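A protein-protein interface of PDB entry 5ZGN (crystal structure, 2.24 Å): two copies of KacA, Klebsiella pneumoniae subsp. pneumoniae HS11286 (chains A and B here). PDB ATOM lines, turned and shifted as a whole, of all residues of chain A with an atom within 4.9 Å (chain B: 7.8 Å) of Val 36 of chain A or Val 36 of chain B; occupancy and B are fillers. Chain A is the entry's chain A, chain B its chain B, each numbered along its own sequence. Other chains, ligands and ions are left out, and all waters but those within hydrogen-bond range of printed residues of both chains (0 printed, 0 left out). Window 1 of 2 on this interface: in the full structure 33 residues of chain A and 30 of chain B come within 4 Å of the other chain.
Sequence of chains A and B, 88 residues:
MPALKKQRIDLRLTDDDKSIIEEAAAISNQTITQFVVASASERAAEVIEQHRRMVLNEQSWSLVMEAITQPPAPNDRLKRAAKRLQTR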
ATOM      1  N   ILE A   9      -6.679  -5.294 -11.038  1.00  0.00           N
ATOM      2  CA  ILE A   9      -7.870  -4.620 -11.501  1.00  0.00           C
ATOM      3  C   ILE A   9      -9.031  -5.189 -10.707  1.00  0.00           C
ATOM      4  O   ILE A   9      -9.087  -6.380 -10.491  1.00  0.00           O
ATOM      5  CB  ILE A   9      -8.129  -4.929 -12.991  1.00  0.00           C
ATOM      6  CG1 ILE A   9      -7.339  -4.031 -13.909  1.00  0.00           C
ATOM      7  CG2 ILE A   9      -9.567  -4.738 -13.385  1.00  0.00           C
ATOM      8  CD1 ILE A   9      -7.425  -4.468 -15.337  1.00  0.00           C
ATOM      9  N   LEU A  11     -13.319  -5.068 -10.397  1.00  0.00           N
ATOM     10  CA  LEU A  11     -14.564  -4.625 -10.965  1.00  0.00           C
ATOM     11  C   LEU A  11     -15.746  -4.787 -10.044  1.00  0.00           C
ATOM     12  O   LEU A  11     -15.933  -5.811  -9.435  1.00  0.00           O
ATOM     13  CB  LEU A  11     -14.867  -5.415 -12.211  1.00  0.00           C
ATOM     14  CG  LEU A  11     -13.676  -5.861 -13.001  1.00  0.00           C
ATOM     15  CD1 LEU A  11     -14.049  -7.038 -13.851  1.00  0.00           C
ATOM     16  CD2 LEU A  11     -13.245  -4.707 -13.858  1.00  0.00           C
ATOM     17  N   ILE A  21     -20.766 -14.085 -16.398  1.00  0.00           N
ATOM     18  CA  ILE A  21     -19.325 -14.223 -16.590  1.00  0.00           C
ATOM     19  C   ILE A  21     -18.812 -15.477 -15.890  1.00  0.00           C
ATOM     20  O   ILE A  21     -18.009 -16.232 -16.450  1.00  0.00           O
ATOM     21  CB  ILE A  21     -18.595 -12.956 -16.105  1.00  0.00           C
ATOM     22  CG1 ILE A  21     -18.818 -11.803 -17.088  1.00  0.00           C
ATOM     23  CG2 ILE A  21     -17.108 -13.225 -15.917  1.00  0.00           C
ATOM     24  CD1 ILE A  21     -18.374 -10.455 -16.561  1.00  0.00           C
ATOM     25  N   ILE A  32     -12.023 -17.445 -13.669  1.00  0.00           N
ATOM     26  CA  ILE A  32     -12.557 -16.109 -13.917  1.00  0.00           C
ATOM     27  C   ILE A  32     -11.470 -15.174 -14.430  1.00  0.00           C
ATOM     28  O   ILE A  32     -11.738 -14.301 -15.265  1.00  0.00           O
ATOM     29  CB  ILE A  32     -13.219 -15.558 -12.637  1.00  0.00           C
ATOM     30  CG1 ILE A  32     -14.223 -16.566 -12.079  1.00  0.00           C
ATOM     31  CG2 ILE A  32     -13.906 -14.228 -12.916  1.00  0.00           C
ATOM     32  CD1 ILE A  32     -15.278 -16.989 -13.075  1.00  0.00           C
ATOM     33  N   THR A  33     -10.230 -15.346 -13.965  1.00  0.00           N
ATOM     34  CA  THR A  33      -9.148 -14.472 -14.405  1.00  0.00           C
ATOM     35  C   THR A  33      -8.842 -14.669 -15.887  1.00  0.00           C
ATOM     36  O   THR A  33      -8.769 -13.697 -16.646  1.00  0.00           O
ATOM     37  CB  THR A  33      -7.896 -14.703 -13.558  1.00  0.00           C
ATOM     38  OG1 THR A  33      -8.146 -14.272 -12.215  1.00  0.00           O
ATOM     39  CG2 THR A  33      -6.725 -13.911 -14.119  1.00  0.00           C
ATOM     40  N   GLN A  34      -8.646 -15.920 -16.315  1.00  0.00           N
ATOM     41  CA  GLN A  34      -8.406 -16.194 -17.732  1.00  0.00           C
ATOM     42  C   GLN A  34      -9.524 -15.626 -18.599  1.00  0.00           C
ATOM     43  O   GLN A  34      -9.271 -14.838 -19.515  1.00  0.00           O
ATOM     44  CB  GLN A  34      -8.250 -17.699 -17.971  1.00  0.00           C
ATOM     45  CG  GLN A  34      -7.649 -18.447 -16.801  1.00  0.00           C
ATOM     46  CD  GLN A  34      -7.314 -19.894 -17.118  1.00  0.00           C
ATOM     47  OE1 GLN A  34      -8.204 -20.695 -17.395  1.00  0.00           O
ATOM     48  NE2 GLN A  34      -6.037 -20.246 -17.031  1.00  0.00           N
ATOM     49  N   PHE A  35     -10.772 -16.011 -18.316  1.00  0.00           N
ATOM     50  CA  PHE A  35     -11.889 -15.594 -19.158  1.00  0.00           C
ATOM     51  C   PHE A  35     -11.991 -14.072 -19.244  1.00  0.00           C
ATOM     52  O   PHE A  35     -12.220 -13.522 -20.325  1.00  0.00           O
ATOM     53  CB  PHE A  35     -13.194 -16.191 -18.632  1.00  0.00           C
ATOM     54  CG  PHE A  35     -14.365 -15.980 -19.550  1.00  0.00           C
ATOM     55  CD1 PHE A  35     -15.141 -14.833 -19.462  1.00  0.00           C
ATOM     56  CD2 PHE A  35     -14.688 -16.929 -20.506  1.00  0.00           C
ATOM     57  CE1 PHE A  35     -16.216 -14.638 -20.311  1.00  0.00           C
ATOM     58  CE2 PHE A  35     -15.761 -16.742 -21.357  1.00  0.00           C
ATOM     59  CZ  PHE A  35     -16.526 -15.595 -21.259  1.00  0.00           C
ATOM     60  N   VAL A  36     -11.821 -13.379 -18.118  1.00  0.00           N
ATOM     61  CA  VAL A  36     -12.043 -11.936 -18.099  1.00  0.00           C
ATOM     62  C   VAL A  36     -10.879 -11.201 -18.754  1.00  0.00           C
ATOM     63  O   VAL A  36     -11.080 -10.327 -19.606  1.00  0.00           O
ATOM     64  CB  VAL A  36     -12.276 -11.453 -16.656  1.00  0.00           C
ATOM     65  CG1 VAL A  36     -12.108  -9.949 -16.564  1.00  0.00           C
ATOM     66  CG2 VAL A  36     -13.661 -11.863 -16.173  1.00  0.00           C
ATOM     67  N   VAL A  37      -9.644 -11.550 -18.385  1.00  0.00           N
ATOM     68  CA  VAL A  37      -8.494 -10.815 -18.903  1.00  0.00           C
ATOM     69  C   VAL A  37      -8.265 -11.137 -20.376  1.00  0.00           C
ATOM     70  O   VAL A  37      -7.904 -10.257 -21.166  1.00  0.00           O
ATOM     71  CB  VAL A  37      -7.246 -11.102 -18.049  1.00  0.00           C
ATOM     72  CG1 VAL A  37      -5.984 -10.602 -18.747  1.00  0.00           C
ATOM     73  CG2 VAL A  37      -7.389 -10.461 -16.675  1.00  0.00           C
ATOM     74  N   ALA A  38      -8.494 -12.390 -20.778  1.00  0.00           N
ATOM     75  CA  ALA A  38      -8.337 -12.733 -22.189  1.00  0.00           C
ATOM     76  C   ALA A  38      -9.384 -12.038 -23.048  1.00  0.00           C
ATOM     77  O   ALA A  38      -9.059 -11.516 -24.119  1.00  0.00           O
ATOM     78  CB  ALA A  38      -8.401 -14.247 -22.388  1.00  0.00           C
ATOM     79  N   SER A  39     -10.643 -12.015 -22.598  1.00  0.00           N
ATOM     80  CA  SER A  39     -11.684 -11.333 -23.362  1.00  0.00           C
ATOM     81  C   SER A  39     -11.377  -9.849 -23.510  1.00  0.00           C
ATOM     82  O   SER A  39     -11.547  -9.274 -24.591  1.00  0.00           O
ATOM     83  CB  SER A  39     -13.046 -11.524 -22.691  1.00  0.00           C
ATOM     84  OG  SER A  39     -13.418 -12.891 -22.651  1.00  0.00           O
ATOM     85  N   ALA A  40     -10.919  -9.214 -22.430  1.00  0.00           N
ATOM     86  CA  ALA A  40     -10.646  -7.783 -22.467  1.00  0.00           C
ATOM     87  C   ALA A  40      -9.399  -7.471 -23.286  1.00  0.00           C
ATOM     88  O   ALA A  40      -9.362  -6.467 -24.008  1.00  0.00           O
ATOM     89  CB  ALA A  40     -10.505  -7.240 -21.044  1.00  0.00           C
ATOM     90  N   ILE B   9     -15.196  -8.655  -8.961  1.00  0.00           N
ATOM     91  CA  ILE B   9     -14.251  -9.547  -9.582  1.00  0.00           C
ATOM     92  C   ILE B   9     -12.884  -8.925  -9.379  1.00  0.00           C
ATOM     93  O   ILE B   9     -12.711  -7.760  -9.623  1.00  0.00           O
ATOM     94  CB  ILE B   9     -14.511  -9.705 -11.075  1.00  0.00           C
ATOM     95  CG1 ILE B   9     -15.685 -10.628 -11.305  1.00  0.00           C
ATOM     96  CG2 ILE B   9     -13.312 -10.289 -11.756  1.00  0.00           C
ATOM     97  CD1 ILE B   9     -15.850 -11.089 -12.721  1.00  0.00           C
ATOM     98  N   ASP B  10     -11.932  -9.694  -8.881  1.00  0.00           N
ATOM     99  CA  ASP B  10     -10.587  -9.214  -8.666  1.00  0.00           C
ATOM    100  C   ASP B  10      -9.666  -9.920  -9.656  1.00  0.00           C
ATOM    101  O   ASP B  10      -9.786 -11.097  -9.843  1.00  0.00           O
ATOM    102  CB  ASP B  10     -10.187  -9.441  -7.228  1.00  0.00           C
ATOM    103  CG  ASP B  10     -11.040  -8.680  -6.256  1.00  0.00           C
ATOM    104  OD1 ASP B  10     -12.139  -9.125  -5.956  1.00  0.00           O
ATOM    105  OD2 ASP B  10     -10.602  -7.652  -5.750  1.00  0.00           O
ATOM    106  N   LEU B  11      -8.746  -9.183 -10.271  1.00  0.00           N
ATOM    107  CA  LEU B  11      -7.877  -9.675 -11.330  1.00  0.00           C
ATOM    108  C   LEU B  11      -6.421  -9.418 -10.985  1.00  0.00           C
ATOM    109  O   LEU B  11      -6.072  -8.357 -10.456  1.00  0.00           O
ATOM    110  CB  LEU B  11      -8.164  -8.996 -12.681  1.00  0.00           C
ATOM    111  CG  LEU B  11      -9.468  -9.143 -13.472  1.00  0.00           C
ATOM    112  CD1 LEU B  11      -9.968 -10.581 -13.481  1.00  0.00           C
ATOM    113  CD2 LEU B  11     -10.529  -8.193 -12.956  1.00  0.00           C
ATOM    114  N   LEU B  13      -2.978  -9.452 -13.454  1.00  0.00           N
ATOM    115  CA  LEU B  13      -2.599  -9.509 -14.859  1.00  0.00           C
ATOM    116  C   LEU B  13      -1.229  -8.876 -15.046  1.00  0.00           C
ATOM    117  O   LEU B  13      -0.722  -8.164 -14.175  1.00  0.00           O
ATOM    118  CB  LEU B  13      -3.635  -8.828 -15.770  1.00  0.00           C
ATOM    119  CG  LEU B  13      -4.517  -7.671 -15.290  1.00  0.00           C
ATOM    120  CD1 LEU B  13      -3.715  -6.550 -14.653  1.00  0.00           C
ATOM    121  CD2 LEU B  13      -5.329  -7.141 -16.462  1.00  0.00           C
ATOM    122  N   ASP B  17      -0.860  -6.692 -20.458  1.00  0.00           N
ATOM    123  CA  ASP B  17      -2.313  -6.756 -20.577  1.00  0.00           C
ATOM    124  C   ASP B  17      -2.973  -5.543 -19.932  1.00  0.00           C
ATOM    125  O   ASP B  17      -3.916  -4.971 -20.490  1.00  0.00           O
ATOM    126  CB  ASP B  17      -2.832  -8.050 -19.955  1.00  0.00           C
ATOM    127  CG  ASP B  17      -2.435  -9.275 -20.750  1.00  0.00           C
ATOM    128  OD1 ASP B  17      -1.994  -9.112 -21.908  1.00  0.00           O
ATOM    129  OD2 ASP B  17      -2.565 -10.400 -20.221  1.00  0.00           O
ATOM    130  N   ILE B  21      -5.149  -2.600 -22.063  1.00  0.00           N
ATOM    131  CA  ILE B  21      -6.537  -2.382 -21.665  1.00  0.00           C
ATOM    132  C   ILE B  21      -6.758  -0.922 -21.288  1.00  0.00           C
ATOM    133  O   ILE B  21      -7.772  -0.317 -21.657  1.00  0.00           O
ATOM    134  CB  ILE B  21      -6.922  -3.335 -20.516  1.00  0.00           C
ATOM    135  CG1 ILE B  21      -7.048  -4.771 -21.028  1.00  0.00           C
ATOM    136  CG2 ILE B  21      -8.224  -2.894 -19.861  1.00  0.00           C
ATOM    137  CD1 ILE B  21      -7.247  -5.797 -19.933  1.00  0.00           C
ATOM    138  N   GLU B  22      -5.810  -0.331 -20.554  1.00  0.00           N
ATOM    139  CA  GLU B  22      -5.928   1.072 -20.167  1.00  0.00           C
ATOM    140  C   GLU B  22      -5.992   1.976 -21.390  1.00  0.00           C
ATOM    141  O   GLU B  22      -6.744   2.958 -21.409  1.00  0.00           O
ATOM    142  CB  GLU B  22      -4.748   1.470 -19.279  1.00  0.00           C
ATOM    143  CG  GLU B  22      -4.851   1.003 -17.836  1.00  0.00           C
ATOM    144  CD  GLU B  22      -3.643   1.407 -17.009  1.00  0.00           C
ATOM    145  OE1 GLU B  22      -2.596   1.737 -17.607  1.00  0.00           O
ATOM    146  OE2 GLU B  22      -3.739   1.398 -15.764  1.00  0.00           O
ATOM    147  N   ALA B  25      -9.286   1.432 -23.339  1.00  0.00           N
ATOM    148  CA  ALA B  25     -10.372   2.100 -22.631  1.00  0.00           C
ATOM    149  C   ALA B  25     -10.337   3.604 -22.872  1.00  0.00           C
ATOM    150  O   ALA B  25     -11.387   4.235 -23.046  1.00  0.00           O
ATOM    151  CB  ALA B  25     -10.293   1.792 -21.136  1.00  0.00           C
ATOM    152  N   GLN B  30     -13.896   5.206 -22.201  1.00  0.00           N
ATOM    153  CA  GLN B  30     -14.503   4.308 -21.230  1.00  0.00           C
ATOM    154  C   GLN B  30     -13.553   4.123 -20.056  1.00  0.00           C
ATOM    155  O   GLN B  30     -12.334   4.180 -20.218  1.00  0.00           O
ATOM    156  CB  GLN B  30     -14.827   2.943 -21.843  1.00  0.00           C
ATOM    157  CG  GLN B  30     -16.245   2.792 -22.348  1.00  0.00           C
ATOM    158  CD  GLN B  30     -16.406   1.584 -23.247  1.00  0.00           C
ATOM    159  OE1 GLN B  30     -15.485   0.781 -23.398  1.00  0.00           O
ATOM    160  NE2 GLN B  30     -17.593   1.426 -23.819  1.00  0.00           N
ATOM    161  N   THR B  31     -14.116   3.916 -18.866  1.00  0.00           N
ATOM    162  CA  THR B  31     -13.285   3.520 -17.738  1.00  0.00           C
ATOM    163  C   THR B  31     -12.712   2.125 -17.976  1.00  0.00           C
ATOM    164  O   THR B  31     -13.162   1.374 -18.846  1.00  0.00           O
ATOM    165  CB  THR B  31     -14.069   3.517 -16.426  1.00  0.00           C
ATOM    166  OG1 THR B  31     -15.193   2.642 -16.542  1.00  0.00           O
ATOM    167  CG2 THR B  31     -14.591   4.912 -16.152  1.00  0.00           C
ATOM    168  N   ILE B  32     -11.703   1.779 -17.176  1.00  0.00           N
ATOM    169  CA  ILE B  32     -11.171   0.421 -17.214  1.00  0.00           C
ATOM    170  C   ILE B  32     -12.268  -0.590 -16.897  1.00  0.00           C
ATOM    171  O   ILE B  32     -12.402  -1.616 -17.577  1.00  0.00           O
ATOM    172  CB  ILE B  32      -9.980   0.284 -16.247  1.00  0.00           C
ATOM    173  CG1 ILE B  32      -8.813   1.162 -16.703  1.00  0.00           C
ATOM    174  CG2 ILE B  32      -9.541  -1.167 -16.138  1.00  0.00           C
ATOM    175  CD1 ILE B  32      -7.738   1.339 -15.647  1.00  0.00           C
ATOM    176  N   THR B  33     -13.085  -0.308 -15.877  1.00  0.00           N
ATOM    177  CA  THR B  33     -14.104  -1.271 -15.466  1.00  0.00           C
ATOM    178  C   THR B  33     -15.188  -1.440 -16.528  1.00  0.00           C
ATOM    179  O   THR B  33     -15.641  -2.563 -16.778  1.00  0.00           O
ATOM    180  CB  THR B  33     -14.707  -0.866 -14.117  1.00  0.00           C
ATOM    181  OG1 THR B  33     -15.835  -1.701 -13.820  1.00  0.00           O
ATOM    182  CG2 THR B  33     -15.150   0.583 -14.127  1.00  0.00           C
ATOM    183  N   GLN B  34     -15.614  -0.345 -17.169  1.00  0.00           N
ATOM    184  CA  GLN B  34     -16.597  -0.450 -18.247  1.00  0.00           C
ATOM    185  C   GLN B  34     -16.056  -1.282 -19.403  1.00  0.00           C
ATOM    186  O   GLN B  34     -16.753  -2.152 -19.937  1.00  0.00           O
ATOM    187  CB  GLN B  34     -17.002   0.940 -18.742  1.00  0.00           C
ATOM    188  CG  GLN B  34     -17.807   1.786 -17.769  1.00  0.00           C
ATOM    189  CD  GLN B  34     -18.055   3.183 -18.313  1.00  0.00           C
ATOM    190  OE1 GLN B  34     -17.111   3.897 -18.649  1.00  0.00           O
ATOM    191  NE2 GLN B  34     -19.319   3.577 -18.400  1.00  0.00           N
ATOM    192  N   PHE B  35     -14.812  -1.017 -19.814  1.00  0.00           N
ATOM    193  CA  PHE B  35     -14.238  -1.737 -20.948  1.00  0.00           C
ATOM    194  C   PHE B  35     -14.103  -3.226 -20.653  1.00  0.00           C
ATOM    195  O   PHE B  35     -14.373  -4.065 -21.520  1.00  0.00           O
ATOM    196  CB  PHE B  35     -12.877  -1.147 -21.319  1.00  0.00           C
ATOM    197  CG  PHE B  35     -12.287  -1.739 -22.569  1.00  0.00           C
ATOM    198  CD1 PHE B  35     -12.559  -1.189 -23.810  1.00  0.00           C
ATOM    199  CD2 PHE B  35     -11.462  -2.851 -22.500  1.00  0.00           C
ATOM    200  CE1 PHE B  35     -12.020  -1.736 -24.960  1.00  0.00           C
ATOM    201  CE2 PHE B  35     -10.923  -3.405 -23.646  1.00  0.00           C
ATOM    202  CZ  PHE B  35     -11.203  -2.846 -24.877  1.00  0.00           C
ATOM    203  N   VAL B  36     -13.683  -3.574 -19.436  1.00  0.00           N
ATOM    204  CA  VAL B  36     -13.439  -4.976 -19.106  1.00  0.00           C
ATOM    205  C   VAL B  36     -14.754  -5.724 -18.930  1.00  0.00           C
ATOM    206  O   VAL B  36     -14.929  -6.834 -19.448  1.00  0.00           O
ATOM    207  CB  VAL B  36     -12.557  -5.080 -17.850  1.00  0.00           C
ATOM    208  CG1 VAL B  36     -12.435  -6.528 -17.408  1.00  0.00           C
ATOM    209  CG2 VAL B  36     -11.181  -4.499 -18.121  1.00  0.00           C
ATOM    210  N   VAL B  37     -15.702  -5.130 -18.199  1.00  0.00           N
ATOM    211  CA  VAL B  37     -16.993  -5.785 -17.987  1.00  0.00           C
ATOM    212  C   VAL B  37     -17.722  -5.972 -19.312  1.00  0.00           C
ATOM    213  O   VAL B  37     -18.309  -7.030 -19.570  1.00  0.00           O
ATOM    214  CB  VAL B  37     -17.840  -4.990 -16.974  1.00  0.00           C
ATOM    215  CG1 VAL B  37     -19.270  -5.521 -16.939  1.00  0.00           C
ATOM    216  CG2 VAL B  37     -17.216  -5.065 -15.590  1.00  0.00           C
ATOM    217  N   ALA B  38     -17.689  -4.955 -20.178  1.00  0.00           N
ATOM    218  CA  ALA B  38     -18.357  -5.072 -21.470  1.00  0.00           C
ATOM    219  C   ALA B  38     -17.697  -6.136 -22.340  1.00  0.00           C
ATOM    220  O   ALA B  38     -18.387  -6.904 -23.019  1.00  0.00           O
ATOM    221  CB  ALA B  38     -18.366  -3.722 -22.186  1.00  0.00           C
ATOM    222  N   SER B  39     -16.364  -6.194 -22.334  1.00  0.00           N
ATOM    223  CA  SER B  39     -15.665  -7.202 -23.124  1.00  0.00           C
ATOM    224  C   SER B  39     -15.944  -8.608 -22.604  1.00  0.00           C
ATOM    225  O   SER B  39     -16.138  -9.542 -23.392  1.00  0.00           O
ATOM    226  CB  SER B  39     -14.164  -6.921 -23.125  1.00  0.00           C
ATOM    227  OG  SER B  39     -13.890  -5.636 -23.655  1.00  0.00           O
ATOM    228  N   ALA B  40     -15.972  -8.780 -21.281  1.00  0.00           N
ATOM    229  CA  ALA B  40     -16.173 -10.109 -20.713  1.00  0.00           C
ATOM    230  C   ALA B  40     -17.624 -10.557 -20.831  1.00  0.00           C
ATOM    231  O   ALA B  40     -17.891 -11.720 -21.153  1.00  0.00           O
ATOM    232  CB  ALA B  40     -15.723 -10.133 -19.252  1.00  0.00           C
ATOM    233  N   SER B  41     -18.574  -9.651 -20.590  1.00  0.00           N
ATOM    234  CA  SER B  41     -19.979 -10.040 -20.631  1.00  0.00           C
ATOM    235  C   SER B  41     -20.458 -10.264 -22.058  1.00  0.00           C
ATOM    236  O   SER B  41     -21.296 -11.141 -22.296  1.00  0.00           O
ATOM    237  CB  SER B  41     -20.842  -8.991 -19.930  1.00  0.00           C
ATOM    238  OG  SER B  41     -20.725  -7.731 -20.562  1.00  0.00           O
ATOM    239  N   GLU B  42     -19.948  -9.484 -23.017  1.00  0.00           N
ATOM    240  CA  GLU B  42     -20.270  -9.734 -24.420  1.00  0.00           C
ATOM    241  C   GLU B  42     -19.740 -11.088 -24.871  1.00  0.00           C
ATOM    242  O   GLU B  42     -20.420 -11.820 -25.601  1.00  0.00           O
ATOM    243  CB  GLU B  42     -19.703  -8.621 -25.302  1.00  0.00           C
ATOM    244  N   ARG B  43     -18.528 -11.446 -24.441  1.00  0.00           N
ATOM    245  CA  ARG B  43     -17.989 -12.749 -24.807  1.00  0.00           C
ATOM    246  C   ARG B  43     -18.687 -13.862 -24.033  1.00  0.00           C
ATOM    247  O   ARG B  43     -18.824 -14.981 -24.541  1.00  0.00           O
ATOM    248  CB  ARG B  43     -16.482 -12.777 -24.549  1.00  0.00           C
ATOM    249  CG  ARG B  43     -15.800 -14.103 -24.846  1.00  0.00           C
ATOM    250  CD  ARG B  43     -15.535 -14.245 -26.338  1.00  0.00           C
ATOM    251  NE  ARG B  43     -14.792 -15.459 -26.659  1.00  0.00           N
ATOM    252  CZ  ARG B  43     -15.291 -16.480 -27.349  1.00  0.00           C
ATOM    253  NH1 ARG B  43     -16.536 -16.432 -27.799  1.00  0.00           N
ATOM    254  NH2 ARG B  43     -14.542 -17.547 -27.595  1.00  0.00           N
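The backbone carbonyl oxygen (O) of Ile 9 of chain A is in hydrogen-bond range of the backbone NH (N) of Leu 11 of chain B (2.8 Å).
The backbone carbonyl oxygen (O) of Ile 9 of chain B lies within hydrogen-bond range of the backbone NH (N) of Leu 11 of chain A, 2.9 Å away.
The backbone carbonyl oxygen (O) of Phe 35 of chain A lies within hydrogen-bond range of the side-chain hydroxyl (OG) of Ser 39 of chain A, at 2.7 Å.
OG of Ser 39 of chain B is in hydrogen-bond range of O of Phe 35 of chain B (2.7 Å).
Among the printed residues, pairs that only touch across the chains: Ile 9 of chain A with Ile 9 of chain B, Ile 9 of chain A with Asp 10 of chain B, Ile 9 of chain A with Leu 13 of chain B, Leu 11 of chain A with Leu 11 of chain B, Leu 11 of chain A with Thr 33 of chain B, Leu 11 of chain A with Val 36 of chain B, Ile 21 of chain A with Ala 40 of chain B, Ile 32 of chain A with Ile 9 of chain B, Phe 35 of chain A with Ala 40 of chain B, Phe 35 of chain A with Arg 43 of chain B, Val 36 of chain A with Leu 11 of chain B, Val 36 of chain A with Val 36 of chain B, Val 37 of chain A with Leu 13 of chain B, Val 37 of chain A with Asp 17 of chain B, Ser 39 of chain A with Ser 39 of chain B, Ser 39 of chain A with Ala 40 of chain B, Ser 39 of chain A with Arg 43 of chain B, Ala 40 of chain A with Ile 21 of chain B, Ala 40 of chain A with Phe 35 of chain B and Ala 40 of chain A with Ser 39 of chain B.
Of the printed residues of chain B, Leu 11 of chain A touches Ile 9 (2.9 Å), Leu 11 (3.8 Å), Thr 33 (3.9 Å) and Val 36 (3.9 Å).
Of the printed residues of chain B, Ile 21 of chain A touches Ala 40 (3.8 Å).
Val 36 of chain A touches two residues of chain B.
Ala 38 of chain A touches none of the printed residues of chain B.
Of the printed residues of chain A, Ile 9 of chain B touches Ile 9, Leu 11 and Ile 32.
Ile 32 of chain B touches none of the printed residues of chain A.
Of the printed residues of chain A, Phe 35 of chain B touches Ala 40 (3.5 Å).
Of chain A, only Leu 11 (3.9 Å) and Val 36 (3.5 Å) come within 4 Å of Val 36 of chain B.
Hydrophobic or aromatic side chains of chain B that line the printed part of chain A: Ile 9, Leu 11, Leu 13, Ile 21, Phe 35, Val 36 and Ala 40.
Printed residues of chain A that touch a printed residue of chain B: Ile 9, Leu 11, Ile 21, Ile 32, Phe 35, Val 36, Val 37, Ser 39 and Ala 40.
Among the printed residues, no Asp or Glu carboxylate lies within 4 Å of a Lys or Arg side-chain nitrogen of the other chain.
Ile 9 of chain A touches Leu 11 of chain B, and with the chains exchanged Leu 11 of chain A touches Ile 9 of chain B.
Ile 32 of chain A touches Ile 9 of chain B, but with the chains exchanged Ile 9 of chain A does not touch Ile 32 of chain B (4.002 Å).
Val 36 of chain B touches its own counterpart, Val 36 of chain A.
Ser 39 of chain A touches Ala 40 of chain B, and with the chains exchanged Ala 40 of chain A touches Ser 39 of chain B.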
